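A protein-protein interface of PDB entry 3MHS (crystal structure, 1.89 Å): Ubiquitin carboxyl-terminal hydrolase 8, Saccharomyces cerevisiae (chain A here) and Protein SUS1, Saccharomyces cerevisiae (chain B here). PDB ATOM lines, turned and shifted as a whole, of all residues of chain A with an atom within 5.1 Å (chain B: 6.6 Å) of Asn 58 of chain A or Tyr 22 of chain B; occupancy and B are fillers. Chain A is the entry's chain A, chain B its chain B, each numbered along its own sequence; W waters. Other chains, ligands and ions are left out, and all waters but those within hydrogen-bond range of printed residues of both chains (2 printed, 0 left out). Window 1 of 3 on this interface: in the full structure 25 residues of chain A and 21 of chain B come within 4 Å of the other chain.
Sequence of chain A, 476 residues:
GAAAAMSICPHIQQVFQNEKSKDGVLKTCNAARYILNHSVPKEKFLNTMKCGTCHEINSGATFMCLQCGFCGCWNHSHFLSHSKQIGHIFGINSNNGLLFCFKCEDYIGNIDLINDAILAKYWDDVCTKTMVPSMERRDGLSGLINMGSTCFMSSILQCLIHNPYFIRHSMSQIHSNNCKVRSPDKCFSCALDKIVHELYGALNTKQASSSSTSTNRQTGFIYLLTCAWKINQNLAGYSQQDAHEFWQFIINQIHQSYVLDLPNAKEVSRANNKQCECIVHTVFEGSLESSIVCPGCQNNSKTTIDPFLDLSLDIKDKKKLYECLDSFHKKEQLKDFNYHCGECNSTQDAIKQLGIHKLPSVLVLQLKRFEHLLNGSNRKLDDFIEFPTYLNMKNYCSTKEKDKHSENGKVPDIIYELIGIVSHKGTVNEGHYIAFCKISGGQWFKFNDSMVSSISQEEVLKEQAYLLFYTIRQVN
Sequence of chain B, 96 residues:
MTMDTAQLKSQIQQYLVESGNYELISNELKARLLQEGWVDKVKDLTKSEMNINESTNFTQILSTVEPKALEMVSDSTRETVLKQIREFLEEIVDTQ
The backbone NH (N) of Ile 57 of chain A sits at hydrogen-bond distance from the side-chain amide oxygen (OE1) of Gln 13 of chain B (2.6 Å).
The side-chain amide oxygen of Asn 58 of chain A sits at hydrogen-bond distance from the side-chain hydroxyl of Tyr 22 of chain B, 2.7 Å away.
O of Met 49 of chain A is in hydrogen-bond range of N of Asn 58 of chain A (3.0 Å).
The side-chain amide oxygen (OD1) of Asn 27 of chain B lies close to the backbone carbonyl oxygen (O) of Glu 23 of chain B (3.3 Å).
The backbone carbonyl oxygen (O) of Leu 16 of chain B is in hydrogen-bond range of the backbone NH (N) of Tyr 22 of chain B.
Phe 45 of chain A touches Val 17 of chain B (CB to CG1, 3.9 Å).
CE1 of Phe 45 of chain A touches CE2 of Tyr 22 of chain B, at 3.5 Å.
Phe 45 of chain A touches Glu 23 of chain B (CE2 to CG, 3.9 Å).
Glu 56 of chain A touches Gln 13 of chain B.
Tyr 22 of chain B touches Ile 57 of chain A (OH to O, 3.8 Å).
Of the printed residues of chain B, Phe 45 of chain A touches Val 17 (3.9 Å), Tyr 22 (3.5 Å) and Glu 23 (3.9 Å).
Printed residues of chain B within 4 Å of Ile 57 of chain A: Gln 13 and Tyr 22.
Of chain B, only Tyr 22 comes within 4 Å of Asn 58 of chain A.
Of the printed residues of chain A, Gln 13 of chain B touches Glu 56 and Ile 57.
Of the printed residues of chain A, Val 17 of chain B touches Phe 45.
Tyr 22 of chain B touches three residues of chain A.
Of the printed residues of chain A, Glu 23 of chain B touches Phe 45 (3.9 Å).
The nearest residue of chain B that does not touch Asn 58 of chain A is Ser 26 of chain B (5.2 Å).
The nearest printed residue of chain A that does not touch Tyr 22 of chain B is Ser 59 of chain A (6.4 Å).
The nearest printed residue of chain A that does not touch Val 17 of chain B is Ile 57 of chain A (4.2 Å).
Printed residues of chain A that touch a printed residue of chain B: Phe 45, Glu 56, Ile 57 and Asn 58.
Along chain A the printed residues that touch a printed residue of chain B span positions 45 to 58.
Among the printed residues, no Asp or Glu carboxylate lies within 4 Å of a Lys or Arg side-chain nitrogen of the other chain.
Water W1 lies within hydrogen-bond range of the side-chain amide oxygen (OD1) of Asn 58 of chain A and the side-chain hydroxyl (OG) of Ser 26 of chain B.
Water W2 bridges the side-chain hydroxyl (OH) of Tyr 22 of chain B and the backbone carbonyl oxygen (O) of Ile 57 of chain A.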
ATOM      1  N   PHE A  45      21.806 -17.252  -7.182  1.00  0.00           N
ATOM      2  CA  PHE A  45      21.198 -16.504  -6.076  1.00  0.00           C
ATOM      3  C   PHE A  45      21.249 -17.272  -4.764  1.00  0.00           C
ATOM      4  O   PHE A  45      21.616 -16.717  -3.707  1.00  0.00           O
ATOM      5  CB  PHE A  45      19.737 -16.116  -6.379  1.00  0.00           C
ATOM      6  CG  PHE A  45      19.595 -14.947  -7.315  1.00  0.00           C
ATOM      7  CD1 PHE A  45      20.128 -13.717  -6.989  1.00  0.00           C
ATOM      8  CD2 PHE A  45      18.863 -15.047  -8.481  1.00  0.00           C
ATOM      9  CE1 PHE A  45      19.989 -12.660  -7.821  1.00  0.00           C
ATOM     10  CE2 PHE A  45      18.725 -13.984  -9.305  1.00  0.00           C
ATOM     11  CZ  PHE A  45      19.290 -12.791  -8.984  1.00  0.00           C
ATOM     12  N   MET A  49      24.743 -15.931  -3.379  1.00  0.00           N
ATOM     13  CA  MET A  49      24.269 -14.616  -2.983  1.00  0.00           C
ATOM     14  C   MET A  49      23.376 -14.634  -1.738  1.00  0.00           C
ATOM     15  O   MET A  49      22.692 -13.659  -1.428  1.00  0.00           O
ATOM     16  CB  MET A  49      23.593 -13.922  -4.134  1.00  0.00           C
ATOM     17  CG  MET A  49      24.588 -13.578  -5.254  1.00  0.00           C
ATOM     18  SD  MET A  49      23.752 -13.045  -6.759  1.00  0.00           S
ATOM     19  CE  MET A  49      25.174 -12.824  -7.853  1.00  0.00           C
ATOM     20  N   GLU A  56      19.718 -13.757   4.124  1.00  0.00           N
ATOM     21  CA  GLU A  56      19.138 -12.865   3.135  1.00  0.00           C
ATOM     22  C   GLU A  56      19.822 -13.040   1.771  1.00  0.00           C
ATOM     23  O   GLU A  56      21.016 -13.376   1.689  1.00  0.00           O
ATOM     24  CB  GLU A  56      19.205 -11.411   3.575  1.00  0.00           C
ATOM     25  CG  GLU A  56      18.235 -11.066   4.704  1.00  0.00           C
ATOM     26  CD  GLU A  56      18.183  -9.582   4.987  1.00  0.00           C
ATOM     27  OE1 GLU A  56      18.366  -9.203   6.159  1.00  0.00           O
ATOM     28  OE2 GLU A  56      17.994  -8.784   4.037  1.00  0.00           O
ATOM     29  N   ILE A  57      19.049 -12.825   0.715  1.00  0.00           N
ATOM     30  CA  ILE A  57      19.595 -12.783  -0.643  1.00  0.00           C
ATOM     31  C   ILE A  57      19.940 -11.337  -0.926  1.00  0.00           C
ATOM     32  O   ILE A  57      19.120 -10.450  -0.691  1.00  0.00           O
ATOM     33  CB  ILE A  57      18.587 -13.276  -1.711  1.00  0.00           C
ATOM     34  CG1 ILE A  57      18.003 -14.657  -1.359  1.00  0.00           C
ATOM     35  CG2 ILE A  57      19.247 -13.296  -3.123  1.00  0.00           C
ATOM     36  CD1 ILE A  57      19.010 -15.755  -1.129  1.00  0.00           C
ATOM     37  N   ASN A  58      21.139 -11.105  -1.458  1.00  0.00           N
ATOM     38  CA  ASN A  58      21.564  -9.772  -1.875  1.00  0.00           C
ATOM     39  C   ASN A  58      21.530  -8.733  -0.722  1.00  0.00           C
ATOM     40  O   ASN A  58      21.063  -7.606  -0.912  1.00  0.00           O
ATOM     41  CB  ASN A  58      20.697  -9.252  -3.027  1.00  0.00           C
ATOM     42  CG  ASN A  58      20.939  -9.974  -4.358  1.00  0.00           C
ATOM     43  OD1 ASN A  58      20.027 -10.063  -5.178  1.00  0.00           O
ATOM     44  ND2 ASN A  58      22.162 -10.437  -4.593  1.00  0.00           N
ATOM     45  N   SER A  59      22.010  -9.122   0.456  1.00  0.00           N
ATOM     46  CA  SER A  59      22.205  -8.176   1.583  1.00  0.00           C
ATOM     47  C   SER A  59      23.483  -7.377   1.324  1.00  0.00           C
ATOM     48  O   SER A  59      24.490  -7.460   2.058  1.00  0.00           O
ATOM     49  CB  SER A  59      22.269  -8.921   2.904  1.00  0.00           C
ATOM     50  OG  SER A  59      22.125  -8.042   4.007  1.00  0.00           O
ATOM     51  N   GLY A  60      23.402  -6.561   0.284  1.00  0.00           N
ATOM     52  CA  GLY A  60      24.571  -6.004  -0.355  1.00  0.00           C
ATOM     53  C   GLY A  60      25.333  -7.109  -1.072  1.00  0.00           C
ATOM     54  O   GLY A  60      24.812  -8.205  -1.268  1.00  0.00           O
ATOM     55  N   THR A  62      27.562 -10.192  -1.655  1.00  0.00           N
ATOM     56  CA  THR A  62      27.806 -11.407  -0.889  1.00  0.00           C
ATOM     57  C   THR A  62      29.191 -11.900  -1.244  1.00  0.00           C
ATOM     58  O   THR A  62      29.580 -11.882  -2.407  1.00  0.00           O
ATOM     59  CB  THR A  62      26.721 -12.472  -1.176  1.00  0.00           C
ATOM     60  OG1 THR A  62      25.451 -11.924  -0.816  1.00  0.00           O
ATOM     61  CG2 THR A  62      26.934 -13.756  -0.354  1.00  0.00           C
ATOM     62  N   ASN A  75      25.995  -5.746   3.904  1.00  0.00           N
ATOM     63  CA  ASN A  75      25.108  -4.817   4.611  1.00  0.00           C
ATOM     64  C   ASN A  75      25.027  -5.033   6.127  1.00  0.00           C
ATOM     65  O   ASN A  75      24.983  -4.054   6.897  1.00  0.00           O
ATOM     66  CB  ASN A  75      23.712  -4.792   3.965  1.00  0.00           C
ATOM     67  CG  ASN A  75      23.699  -4.057   2.611  1.00  0.00           C
ATOM     68  OD1 ASN A  75      22.639  -3.804   2.034  1.00  0.00           O
ATOM     69  ND2 ASN A  75      24.864  -3.682   2.135  1.00  0.00           N
ATOM     70  N   ASN A  95      29.019 -11.099  -7.359  1.00  0.00           N
ATOM     71  CA  ASN A  95      28.568 -10.351  -8.540  1.00  0.00           C
ATOM     72  C   ASN A  95      29.630 -10.099  -9.592  1.00  0.00           C
ATOM     73  O   ASN A  95      29.289  -9.796 -10.748  1.00  0.00           O
ATOM     74  CB  ASN A  95      27.986  -8.999  -8.134  1.00  0.00           C
ATOM     75  CG  ASN A  95      26.659  -9.119  -7.461  1.00  0.00           C
ATOM     76  OD1 ASN A  95      25.663  -9.468  -8.098  1.00  0.00           O
ATOM     77  ND2 ASN A  95      26.613  -8.784  -6.178  1.00  0.00           N
ATOM     78  N   ILE B  12      10.751 -15.128   2.551  1.00  0.00           N
ATOM     79  CA  ILE B  12      10.111 -14.494   1.410  1.00  0.00           C
ATOM     80  C   ILE B  12      11.050 -14.411   0.195  1.00  0.00           C
ATOM     81  O   ILE B  12      10.642 -14.709  -0.918  1.00  0.00           O
ATOM     82  CB  ILE B  12       9.584 -13.086   1.798  1.00  0.00           C
ATOM     83  CG1 ILE B  12       8.391 -13.232   2.762  1.00  0.00           C
ATOM     84  CG2 ILE B  12       9.235 -12.264   0.540  1.00  0.00           C
ATOM     85  CD1 ILE B  12       7.874 -11.922   3.350  1.00  0.00           C
ATOM     86  N   GLN B  13      12.302 -14.031   0.420  1.00  0.00           N
ATOM     87  CA  GLN B  13      13.275 -13.939  -0.648  1.00  0.00           C
ATOM     88  C   GLN B  13      13.551 -15.277  -1.311  1.00  0.00           C
ATOM     89  O   GLN B  13      13.718 -15.335  -2.526  1.00  0.00           O
ATOM     90  CB  GLN B  13      14.586 -13.356  -0.137  1.00  0.00           C
ATOM     91  CG  GLN B  13      14.517 -11.895   0.195  1.00  0.00           C
ATOM     92  CD  GLN B  13      15.556 -11.481   1.220  1.00  0.00           C
ATOM     93  OE1 GLN B  13      16.621 -12.085   1.334  1.00  0.00           O
ATOM     94  NE2 GLN B  13      15.244 -10.443   1.973  1.00  0.00           N
ATOM     95  N   GLN B  14      13.653 -16.331  -0.510  1.00  0.00           N
ATOM     96  CA  GLN B  14      13.857 -17.676  -1.035  1.00  0.00           C
ATOM     97  C   GLN B  14      12.726 -18.081  -1.969  1.00  0.00           C
ATOM     98  O   GLN B  14      12.996 -18.623  -3.061  1.00  0.00           O
ATOM     99  CB  GLN B  14      13.981 -18.695   0.094  1.00  0.00           C
ATOM    100  CG  GLN B  14      14.258 -20.138  -0.356  1.00  0.00           C
ATOM    101  CD  GLN B  14      15.741 -20.485  -0.382  1.00  0.00           C
ATOM    102  OE1 GLN B  14      16.132 -21.563  -0.844  1.00  0.00           O
ATOM    103  NE2 GLN B  14      16.571 -19.588   0.145  1.00  0.00           N
ATOM    104  N   TYR B  15      11.473 -17.862  -1.537  1.00  0.00           N
ATOM    105  CA  TYR B  15      10.304 -18.080  -2.391  1.00  0.00           C
ATOM    106  C   TYR B  15      10.356 -17.287  -3.681  1.00  0.00           C
ATOM    107  O   TYR B  15      10.043 -17.822  -4.751  1.00  0.00           O
ATOM    108  CB  TYR B  15       8.981 -17.711  -1.705  1.00  0.00           C
ATOM    109  CG  TYR B  15       7.958 -17.349  -2.760  1.00  0.00           C
ATOM    110  CD1 TYR B  15       7.349 -18.338  -3.530  1.00  0.00           C
ATOM    111  CD2 TYR B  15       7.700 -16.027  -3.077  1.00  0.00           C
ATOM    112  CE1 TYR B  15       6.464 -18.021  -4.535  1.00  0.00           C
ATOM    113  CE2 TYR B  15       6.821 -15.695  -4.085  1.00  0.00           C
ATOM    114  CZ  TYR B  15       6.198 -16.695  -4.811  1.00  0.00           C
ATOM    115  OH  TYR B  15       5.322 -16.360  -5.821  1.00  0.00           O
ATOM    116  N   LEU B  16      10.690 -15.999  -3.596  1.00  0.00           N
ATOM    117  CA  LEU B  16      10.815 -15.176  -4.798  1.00  0.00           C
ATOM    118  C   LEU B  16      11.831 -15.777  -5.781  1.00  0.00           C
ATOM    119  O   LEU B  16      11.587 -15.778  -6.986  1.00  0.00           O
ATOM    120  CB  LEU B  16      11.184 -13.723  -4.476  1.00  0.00           C
ATOM    121  CG  LEU B  16      10.097 -12.822  -3.866  1.00  0.00           C
ATOM    122  CD1 LEU B  16      10.659 -11.402  -3.735  1.00  0.00           C
ATOM    123  CD2 LEU B  16       8.854 -12.799  -4.732  1.00  0.00           C
ATOM    124  N   VAL B  17      12.960 -16.275  -5.283  1.00  0.00           N
ATOM    125  CA  VAL B  17      13.972 -16.866  -6.150  1.00  0.00           C
ATOM    126  C   VAL B  17      13.491 -18.192  -6.762  1.00  0.00           C
ATOM    127  O   VAL B  17      13.654 -18.438  -7.961  1.00  0.00           O
ATOM    128  CB  VAL B  17      15.319 -17.109  -5.411  1.00  0.00           C
ATOM    129  CG1 VAL B  17      16.295 -17.848  -6.325  1.00  0.00           C
ATOM    130  CG2 VAL B  17      15.927 -15.773  -4.884  1.00  0.00           C
ATOM    131  N   GLU B  18      12.920 -19.060  -5.945  1.00  0.00           N
ATOM    132  CA  GLU B  18      12.488 -20.366  -6.437  1.00  0.00           C
ATOM    133  C   GLU B  18      11.363 -20.241  -7.448  1.00  0.00           C
ATOM    134  O   GLU B  18      11.300 -21.029  -8.409  1.00  0.00           O
ATOM    135  CB  GLU B  18      12.128 -21.303  -5.276  1.00  0.00           C
ATOM    136  CG  GLU B  18      13.377 -21.948  -4.680  1.00  0.00           C
ATOM    137  CD  GLU B  18      13.158 -22.600  -3.335  1.00  0.00           C
ATOM    138  OE1 GLU B  18      12.172 -22.274  -2.635  1.00  0.00           O
ATOM    139  OE2 GLU B  18      14.008 -23.432  -2.956  1.00  0.00           O
ATOM    140  N   SER B  19      10.528 -19.209  -7.282  1.00  0.00           N
ATOM    141  CA  SER B  19       9.373 -18.977  -8.166  1.00  0.00           C
ATOM    142  C   SER B  19       9.716 -18.381  -9.535  1.00  0.00           C
ATOM    143  O   SER B  19       8.858 -18.335 -10.416  1.00  0.00           O
ATOM    144  CB  SER B  19       8.362 -18.059  -7.482  1.00  0.00           C
ATOM    145  OG  SER B  19       8.861 -16.737  -7.390  1.00  0.00           O
ATOM    146  N   GLY B  20      10.945 -17.897  -9.694  1.00  0.00           N
ATOM    147  CA  GLY B  20      11.360 -17.199 -10.902  1.00  0.00           C
ATOM    148  C   GLY B  20      11.141 -15.700 -10.821  1.00  0.00           C
ATOM    149  O   GLY B  20      11.610 -14.953 -11.634  1.00  0.00           O
ATOM    150  N   ASN B  21      10.432 -15.231  -9.806  1.00  0.00           N
ATOM    151  CA  ASN B  21      10.055 -13.838  -9.766  1.00  0.00           C
ATOM    152  C   ASN B  21      11.149 -12.924  -9.278  1.00  0.00           C
ATOM    153  O   ASN B  21      11.175 -11.741  -9.638  1.00  0.00           O
ATOM    154  CB  ASN B  21       8.778 -13.663  -8.946  1.00  0.00           C
ATOM    155  CG  ASN B  21       7.586 -14.279  -9.630  1.00  0.00           C
ATOM    156  OD1 ASN B  21       7.510 -14.304 -10.869  1.00  0.00           O
ATOM    157  ND2 ASN B  21       6.696 -14.857  -8.849  1.00  0.00           N
ATOM    158  N   TYR B  22      12.092 -13.454  -8.509  1.00  0.00           N
ATOM    159  CA  TYR B  22      13.248 -12.636  -8.100  1.00  0.00           C
ATOM    160  C   TYR B  22      14.047 -12.180  -9.296  1.00  0.00           C
ATOM    161  O   TYR B  22      14.463 -11.036  -9.388  1.00  0.00           O
ATOM    162  CB  TYR B  22      14.170 -13.397  -7.152  1.00  0.00           C
ATOM    163  CG  TYR B  22      15.066 -12.480  -6.358  1.00  0.00           C
ATOM    164  CD1 TYR B  22      14.634 -11.946  -5.149  1.00  0.00           C
ATOM    165  CD2 TYR B  22      16.366 -12.211  -6.768  1.00  0.00           C
ATOM    166  CE1 TYR B  22      15.447 -11.133  -4.406  1.00  0.00           C
ATOM    167  CE2 TYR B  22      17.204 -11.395  -6.033  1.00  0.00           C
ATOM    168  CZ  TYR B  22      16.738 -10.864  -4.832  1.00  0.00           C
ATOM    169  OH  TYR B  22      17.524 -10.052  -4.061  1.00  0.00           O
ATOM    170  N   GLU B  23      14.269 -13.098 -10.225  1.00  0.00           N
ATOM    171  CA  GLU B  23      14.908 -12.772 -11.488  1.00  0.00           C
ATOM    172  C   GLU B  23      14.149 -11.692 -12.236  1.00  0.00           C
ATOM    173  O   GLU B  23      14.756 -10.803 -12.777  1.00  0.00           O
ATOM    174  CB  GLU B  23      14.968 -13.997 -12.375  1.00  0.00           C
ATOM    175  CG  GLU B  23      16.027 -14.972 -12.005  1.00  0.00           C
ATOM    176  CD  GLU B  23      15.794 -16.298 -12.683  1.00  0.00           C
ATOM    177  OE1 GLU B  23      16.157 -16.439 -13.881  1.00  0.00           O
ATOM    178  OE2 GLU B  23      15.221 -17.182 -12.019  1.00  0.00           O
ATOM    179  N   LEU B  24      12.833 -11.811 -12.350  1.00  0.00           N
ATOM    180  CA  LEU B  24      12.052 -10.805 -13.079  1.00  0.00           C
ATOM    181  C   LEU B  24      12.226  -9.419 -12.456  1.00  0.00           C
ATOM    182  O   LEU B  24      12.369  -8.404 -13.162  1.00  0.00           O
ATOM    183  CB  LEU B  24      10.562 -11.157 -13.055  1.00  0.00           C
ATOM    184  CG  LEU B  24      10.154 -12.413 -13.820  1.00  0.00           C
ATOM    185  CD1 LEU B  24       8.631 -12.611 -13.689  1.00  0.00           C
ATOM    186  CD2 LEU B  24      10.602 -12.285 -15.303  1.00  0.00           C
ATOM    187  N   ILE B  25      12.198  -9.368 -11.130  1.00  0.00           N
ATOM    188  CA  ILE B  25      12.351  -8.090 -10.433  1.00  0.00           C
ATOM    189  C   ILE B  25      13.767  -7.530 -10.632  1.00  0.00           C
ATOM    190  O   ILE B  25      13.951  -6.375 -10.950  1.00  0.00           O
ATOM    191  CB  ILE B  25      12.137  -8.218  -8.918  1.00  0.00           C
ATOM    192  CG1 ILE B  25      10.697  -8.607  -8.592  1.00  0.00           C
ATOM    193  CG2 ILE B  25      12.513  -6.908  -8.255  1.00  0.00           C
ATOM    194  CD1 ILE B  25      10.512  -9.243  -7.180  1.00  0.00           C
ATOM    195  N   SER B  26      14.750  -8.361 -10.351  1.00  0.00           N
ATOM    196  CA  SER B  26      16.148  -7.958 -10.437  1.00  0.00           C
ATOM    197  C   SER B  26      16.490  -7.483 -11.855  1.00  0.00           C
ATOM    198  O   SER B  26      17.112  -6.424 -12.008  1.00  0.00           O
ATOM    199  CB  SER B  26      17.067  -9.111 -10.022  1.00  0.00           C
ATOM    200  OG  SER B  26      18.409  -8.658  -9.921  1.00  0.00           O
ATOM    201  N   ASN B  27      16.042  -8.244 -12.858  1.00  0.00           N
ATOM    202  CA  ASN B  27      16.297  -7.949 -14.271  1.00  0.00           C
ATOM    203  C   ASN B  27      15.572  -6.666 -14.726  1.00  0.00           C
ATOM    204  O   ASN B  27      16.157  -5.843 -15.410  1.00  0.00           O
ATOM    205  CB  ASN B  27      15.846  -9.105 -15.155  1.00  0.00           C
ATOM    206  CG  ASN B  27      16.728 -10.380 -15.014  1.00  0.00           C
ATOM    207  OD1 ASN B  27      16.380 -11.428 -15.542  1.00  0.00           O
ATOM    208  ND2 ASN B  27      17.799 -10.288 -14.295  1.00  0.00           N
ATOM    209  N   PHE B  88       3.967  -9.412  -6.371  1.00  0.00           N
ATOM    210  CA  PHE B  88       4.503 -10.747  -6.142  1.00  0.00           C
ATOM    211  C   PHE B  88       4.406 -11.138  -4.671  1.00  0.00           C
ATOM    212  O   PHE B  88       4.252 -12.314  -4.368  1.00  0.00           O
ATOM    213  CB  PHE B  88       5.967 -10.860  -6.591  1.00  0.00           C
ATOM    214  CG  PHE B  88       6.168 -10.766  -8.083  1.00  0.00           C
ATOM    215  CD1 PHE B  88       5.269 -11.333  -8.961  1.00  0.00           C
ATOM    216  CD2 PHE B  88       7.303 -10.163  -8.600  1.00  0.00           C
ATOM    217  CE1 PHE B  88       5.467 -11.260 -10.314  1.00  0.00           C
ATOM    218  CE2 PHE B  88       7.511 -10.098  -9.964  1.00  0.00           C
ATOM    219  CZ  PHE B  88       6.586 -10.639 -10.818  1.00  0.00           C
HETATM  220  O   HOH W   1      20.241  -8.782  -7.702  1.00  0.00           O
HETATM  221  O   HOH W   2      16.358  -9.086  -1.626  1.00  0.00           O
